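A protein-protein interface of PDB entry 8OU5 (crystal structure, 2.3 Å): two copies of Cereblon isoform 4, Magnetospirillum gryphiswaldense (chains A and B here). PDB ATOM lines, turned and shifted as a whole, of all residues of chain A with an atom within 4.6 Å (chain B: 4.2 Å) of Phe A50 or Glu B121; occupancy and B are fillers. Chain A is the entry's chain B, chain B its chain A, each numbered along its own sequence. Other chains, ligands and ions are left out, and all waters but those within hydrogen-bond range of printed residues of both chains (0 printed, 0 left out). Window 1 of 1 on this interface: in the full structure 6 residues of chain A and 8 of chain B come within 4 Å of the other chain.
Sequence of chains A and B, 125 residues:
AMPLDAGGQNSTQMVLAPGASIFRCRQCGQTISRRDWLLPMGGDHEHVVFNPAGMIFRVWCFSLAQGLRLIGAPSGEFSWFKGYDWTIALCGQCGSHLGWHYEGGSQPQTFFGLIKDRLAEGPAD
Printed residues of chain B within 4 Å of Val A48: Ala B120 and Glu B121.
Ile A56 touches none of the printed residues of chain B.
Ser B21 touches none of the printed residues of chain A.
Of the printed residues of chain A, Ile B22 touches Phe A50 (3.6 Å).
Of the printed residues of chain A, Ala B120 touches Val A48 and Phe A50.
Of chain A, only Val A48, Val A49 and Phe A50 come within 4 Å of Glu B121.
Of the printed residues of chain A, Pro B123 touches Phe A50 (3.4 Å).
The nearest printed residue of chain B that does not touch Phe A50 is Phe B23 (5.0 Å).
N of Ser B21 sits at hydrogen-bond distance from O of Gly B122 (2.8 Å).
N of Ile B22 sits at hydrogen-bond distance from O of Gly B122, 2.8 Å away.
O of Arg B24 is in hydrogen-bond range of N of Ala B120 (2.8 Å).
NE of Arg B35 is in salt-bridge range of OE2 of Glu B121.
The indole nitrogen (NE1) of Trp A80 sits at hydrogen-bond distance from the backbone carbonyl oxygen (O) of Phe A50, 2.9 Å away.
Of the 8 printed residues of chain A, 3 touch a printed residue of chain B.
Hydrophobic or aromatic side chains of chain A within 4 Å of the printed part of chain B: Val A48, Val A49 and Phe A50.
Hydrophobic or aromatic side chains of chain B that line the printed part of chain A: Ile B22, Ala B120 and Pro B123.
Among the printed residues, pairs that only touch across the chains: Val A48 with Ala B120 (3.4 Å), Val A49 with Glu B121 (3.0 Å), Phe A50 with Ile B22 (3.6 Å), Phe A50 with Arg B24 (3.4 Å), Phe A50 with Ala B120 (3.4 Å), Phe A50 with Gly B122 (3.1 Å) and Phe A50 with Pro B123 (3.4 Å).
O of Val A48 is in hydrogen-bond range of N of Glu B121.
The backbone carbonyl oxygen (O) of Glu B121 is in hydrogen-bond range of the backbone NH (N) of Phe A50 (3.0 Å).
No position is printed for both chains.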
ATOM      1  N   VAL A  48      14.215 -14.147  11.993  1.00  0.00           N
ATOM      2  CA  VAL A  48      13.654 -12.817  11.799  1.00  0.00           C
ATOM      3  C   VAL A  48      12.948 -12.792  10.444  1.00  0.00           C
ATOM      4  O   VAL A  48      13.565 -13.078   9.420  1.00  0.00           O
ATOM      5  CB  VAL A  48      14.737 -11.727  11.907  1.00  0.00           C
ATOM      6  CG1 VAL A  48      14.159 -10.330  11.729  1.00  0.00           C
ATOM      7  CG2 VAL A  48      15.497 -11.821  13.224  1.00  0.00           C
ATOM      8  N   VAL A  49      11.647 -12.468  10.456  1.00  0.00           N
ATOM      9  CA  VAL A  49      10.806 -12.594   9.274  1.00  0.00           C
ATOM     10  C   VAL A  49       9.979 -11.323   9.093  1.00  0.00           C
ATOM     11  O   VAL A  49       9.800 -10.557  10.033  1.00  0.00           O
ATOM     12  CB  VAL A  49       9.911 -13.842   9.356  1.00  0.00           C
ATOM     13  CG1 VAL A  49      10.714 -15.125   9.301  1.00  0.00           C
ATOM     14  CG2 VAL A  49       9.043 -13.836  10.596  1.00  0.00           C
ATOM     15  N   PHE A  50       9.508 -11.093   7.863  1.00  0.00           N
ATOM     16  CA  PHE A  50       8.539 -10.042   7.587  1.00  0.00           C
ATOM     17  C   PHE A  50       7.340 -10.631   6.845  1.00  0.00           C
ATOM     18  O   PHE A  50       7.485 -11.518   6.009  1.00  0.00           O
ATOM     19  CB  PHE A  50       9.155  -8.886   6.794  1.00  0.00           C
ATOM     20  CG  PHE A  50       9.604  -9.225   5.393  1.00  0.00           C
ATOM     21  CD1 PHE A  50       8.732  -9.097   4.321  1.00  0.00           C
ATOM     22  CD2 PHE A  50      10.903  -9.635   5.136  1.00  0.00           C
ATOM     23  CE1 PHE A  50       9.139  -9.405   3.033  1.00  0.00           C
ATOM     24  CE2 PHE A  50      11.310  -9.940   3.848  1.00  0.00           C
ATOM     25  CZ  PHE A  50      10.428  -9.829   2.799  1.00  0.00           C
ATOM     26  N   ASN A  51       6.146 -10.115   7.159  1.00  0.00           N
ATOM     27  CA  ASN A  51       4.911 -10.542   6.523  1.00  0.00           C
ATOM     28  C   ASN A  51       4.652  -9.648   5.313  1.00  0.00           C
ATOM     29  O   ASN A  51       5.387  -8.689   5.095  1.00  0.00           O
ATOM     30  CB  ASN A  51       3.760 -10.564   7.538  1.00  0.00           C
ATOM     31  CG  ASN A  51       3.293  -9.197   7.992  1.00  0.00           C
ATOM     32  OD1 ASN A  51       3.573  -8.177   7.361  1.00  0.00           O
ATOM     33  ND2 ASN A  51       2.561  -9.178   9.094  1.00  0.00           N
ATOM     34  N   PRO A  52       3.621  -9.920   4.478  1.00  0.00           N
ATOM     35  CA  PRO A  52       3.365  -9.118   3.280  1.00  0.00           C
ATOM     36  C   PRO A  52       2.935  -7.677   3.539  1.00  0.00           C
ATOM     37  O   PRO A  52       2.925  -6.877   2.609  1.00  0.00           O
ATOM     38  CB  PRO A  52       2.233  -9.854   2.547  1.00  0.00           C
ATOM     39  CG  PRO A  52       2.191 -11.224   3.176  1.00  0.00           C
ATOM     40  CD  PRO A  52       2.678 -11.037   4.597  1.00  0.00           C
ATOM     41  N   MET A  55       5.470  -5.943   8.243  1.00  0.00           N
ATOM     42  CA  MET A  55       5.707  -6.034   9.676  1.00  0.00           C
ATOM     43  C   MET A  55       6.825  -7.045   9.909  1.00  0.00           C
ATOM     44  O   MET A  55       6.796  -8.121   9.319  1.00  0.00           O
ATOM     45  CB  MET A  55       4.452  -6.518  10.408  1.00  0.00           C
ATOM     46  CG  MET A  55       3.269  -5.562  10.322  1.00  0.00           C
ATOM     47  SD  MET A  55       1.704  -6.337  10.843  1.00  0.00           S
ATOM     48  CE  MET A  55       0.521  -5.215  10.103  1.00  0.00           C
ATOM     49  N   ILE A  56       7.803  -6.691  10.753  1.00  0.00           N
ATOM     50  CA  ILE A  56       8.930  -7.554  11.059  1.00  0.00           C
ATOM     51  C   ILE A  56       8.741  -8.153  12.451  1.00  0.00           C
ATOM     52  O   ILE A  56       8.353  -7.451  13.377  1.00  0.00           O
ATOM     53  CB  ILE A  56      10.258  -6.776  10.943  1.00  0.00           C
ATOM     54  CG1 ILE A  56      10.532  -6.348   9.501  1.00  0.00           C
ATOM     55  CG2 ILE A  56      11.422  -7.586  11.504  1.00  0.00           C
ATOM     56  CD1 ILE A  56      11.606  -5.293   9.367  1.00  0.00           C
ATOM     57  N   TRP A  80       6.168 -18.742   6.120  1.00  0.00           N
ATOM     58  CA  TRP A  80       7.612 -18.597   6.253  1.00  0.00           C
ATOM     59  C   TRP A  80       8.314 -19.955   6.244  1.00  0.00           C
ATOM     60  O   TRP A  80       9.527 -20.015   6.068  1.00  0.00           O
ATOM     61  CB  TRP A  80       7.976 -17.823   7.527  1.00  0.00           C
ATOM     62  CG  TRP A  80       7.538 -16.395   7.536  1.00  0.00           C
ATOM     63  CD1 TRP A  80       7.752 -15.458   6.569  1.00  0.00           C
ATOM     64  CD2 TRP A  80       6.807 -15.736   8.582  1.00  0.00           C
ATOM     65  NE1 TRP A  80       7.182 -14.269   6.930  1.00  0.00           N
ATOM     66  CE2 TRP A  80       6.597 -14.407   8.162  1.00  0.00           C
ATOM     67  CE3 TRP A  80       6.302 -16.141   9.820  1.00  0.00           C
ATOM     68  CZ2 TRP A  80       5.902 -13.483   8.944  1.00  0.00           C
ATOM     69  CZ3 TRP A  80       5.608 -15.233  10.590  1.00  0.00           C
ATOM     70  CH2 TRP A  80       5.417 -13.919  10.159  1.00  0.00           C
ATOM     71  N   SER B  21      11.570 -15.917   1.072  1.00  0.00           N
ATOM     72  CA  SER B  21      12.419 -16.152  -0.122  1.00  0.00           C
ATOM     73  C   SER B  21      13.322 -14.960  -0.423  1.00  0.00           C
ATOM     74  O   SER B  21      14.294 -15.155  -1.149  1.00  0.00           O
ATOM     75  CB  SER B  21      11.593 -16.515  -1.326  1.00  0.00           C
ATOM     76  OG  SER B  21      10.772 -15.428  -1.719  1.00  0.00           O
ATOM     77  N   ILE B  22      13.050 -13.761   0.127  1.00  0.00           N
ATOM     78  CA  ILE B  22      13.988 -12.659  -0.028  1.00  0.00           C
ATOM     79  C   ILE B  22      14.384 -12.110   1.339  1.00  0.00           C
ATOM     80  O   ILE B  22      13.628 -12.224   2.292  1.00  0.00           O
ATOM     81  CB  ILE B  22      13.441 -11.542  -0.937  1.00  0.00           C
ATOM     82  CG1 ILE B  22      12.473 -10.614  -0.205  1.00  0.00           C
ATOM     83  CG2 ILE B  22      12.818 -12.116  -2.200  1.00  0.00           C
ATOM     84  CD1 ILE B  22      12.150  -9.360  -0.979  1.00  0.00           C
ATOM     85  N   PHE B  23      15.565 -11.491   1.392  1.00  0.00           N
ATOM     86  CA  PHE B  23      16.105 -10.916   2.609  1.00  0.00           C
ATOM     87  C   PHE B  23      16.091  -9.397   2.498  1.00  0.00           C
ATOM     88  O   PHE B  23      16.596  -8.833   1.529  1.00  0.00           O
ATOM     89  CB  PHE B  23      17.521 -11.434   2.866  1.00  0.00           C
ATOM     90  CG  PHE B  23      17.589 -12.914   3.129  1.00  0.00           C
ATOM     91  CD1 PHE B  23      17.236 -13.440   4.363  1.00  0.00           C
ATOM     92  CD2 PHE B  23      17.997 -13.779   2.133  1.00  0.00           C
ATOM     93  CE1 PHE B  23      17.295 -14.804   4.594  1.00  0.00           C
ATOM     94  CE2 PHE B  23      18.056 -15.146   2.367  1.00  0.00           C
ATOM     95  CZ  PHE B  23      17.692 -15.656   3.591  1.00  0.00           C
ATOM     96  N   ARG B  24      15.531  -8.766   3.537  1.00  0.00           N
ATOM     97  CA  ARG B  24      15.525  -7.324   3.662  1.00  0.00           C
ATOM     98  C   ARG B  24      16.348  -6.925   4.883  1.00  0.00           C
ATOM     99  O   ARG B  24      16.629  -7.744   5.752  1.00  0.00           O
ATOM    100  CB  ARG B  24      14.085  -6.827   3.781  1.00  0.00           C
ATOM    101  CG  ARG B  24      13.257  -7.035   2.519  1.00  0.00           C
ATOM    102  CD  ARG B  24      11.812  -6.594   2.655  1.00  0.00           C
ATOM    103  NE  ARG B  24      11.087  -6.781   1.404  1.00  0.00           N
ATOM    104  CZ  ARG B  24      11.303  -6.090   0.286  1.00  0.00           C
ATOM    105  NH1 ARG B  24      12.063  -5.010   0.302  1.00  0.00           N
ATOM    106  NH2 ARG B  24      10.717  -6.465  -0.839  1.00  0.00           N
ATOM    107  N   ARG B  35      17.248 -16.034  -1.099  1.00  0.00           N
ATOM    108  CA  ARG B  35      17.631 -17.348  -0.605  1.00  0.00           C
ATOM    109  C   ARG B  35      18.280 -18.134  -1.744  1.00  0.00           C
ATOM    110  O   ARG B  35      19.251 -18.855  -1.532  1.00  0.00           O
ATOM    111  CB  ARG B  35      16.416 -18.055   0.017  1.00  0.00           C
ATOM    112  CG  ARG B  35      16.686 -19.470   0.513  1.00  0.00           C
ATOM    113  CD  ARG B  35      15.656 -19.971   1.514  1.00  0.00           C
ATOM    114  NE  ARG B  35      15.908 -19.546   2.889  1.00  0.00           N
ATOM    115  CZ  ARG B  35      16.789 -20.100   3.725  1.00  0.00           C
ATOM    116  NH1 ARG B  35      17.493 -21.162   3.373  1.00  0.00           N
ATOM    117  NH2 ARG B  35      16.951 -19.584   4.932  1.00  0.00           N
ATOM    118  N   ALA B 120      16.005  -9.798   7.569  1.00  0.00           N
ATOM    119  CA  ALA B 120      14.654 -10.295   7.792  1.00  0.00           C
ATOM    120  C   ALA B 120      14.182 -11.022   6.534  1.00  0.00           C
ATOM    121  O   ALA B 120      14.215 -10.442   5.451  1.00  0.00           O
ATOM    122  CB  ALA B 120      13.719  -9.158   8.145  1.00  0.00           C
ATOM    123  N   GLU B 121      13.764 -12.285   6.687  1.00  0.00           N
ATOM    124  CA  GLU B 121      13.403 -13.109   5.549  1.00  0.00           C
ATOM    125  C   GLU B 121      11.891 -13.041   5.353  1.00  0.00           C
ATOM    126  O   GLU B 121      11.145 -13.005   6.324  1.00  0.00           O
ATOM    127  CB  GLU B 121      13.858 -14.557   5.745  1.00  0.00           C
ATOM    128  CG  GLU B 121      13.730 -15.395   4.478  1.00  0.00           C
ATOM    129  CD  GLU B 121      14.133 -16.858   4.587  1.00  0.00           C
ATOM    130  OE1 GLU B 121      14.371 -17.329   5.722  1.00  0.00           O
ATOM    131  OE2 GLU B 121      14.227 -17.523   3.524  1.00  0.00           O
ATOM    132  N   GLY B 122      11.450 -13.035   4.094  1.00  0.00           N
ATOM    133  CA  GLY B 122      10.029 -12.987   3.808  1.00  0.00           C
ATOM    134  C   GLY B 122       9.713 -13.105   2.321  1.00  0.00           C
ATOM    135  O   GLY B 122      10.611 -13.268   1.491  1.00  0.00           O
ATOM    136  N   PRO B 123       8.407 -13.059   1.966  1.00  0.00           N
ATOM    137  CA  PRO B 123       7.951 -13.332   0.602  1.00  0.00           C
ATOM    138  C   PRO B 123       8.384 -12.287  -0.423  1.00  0.00           C
ATOM    139  O   PRO B 123       8.647 -11.136  -0.081  1.00  0.00           O
ATOM    140  CB  PRO B 123       6.415 -13.375   0.726  1.00  0.00           C
ATOM    141  CG  PRO B 123       6.106 -12.566   1.971  1.00  0.00           C
ATOM    142  CD  PRO B 123       7.292 -12.783   2.886  1.00  0.00           C
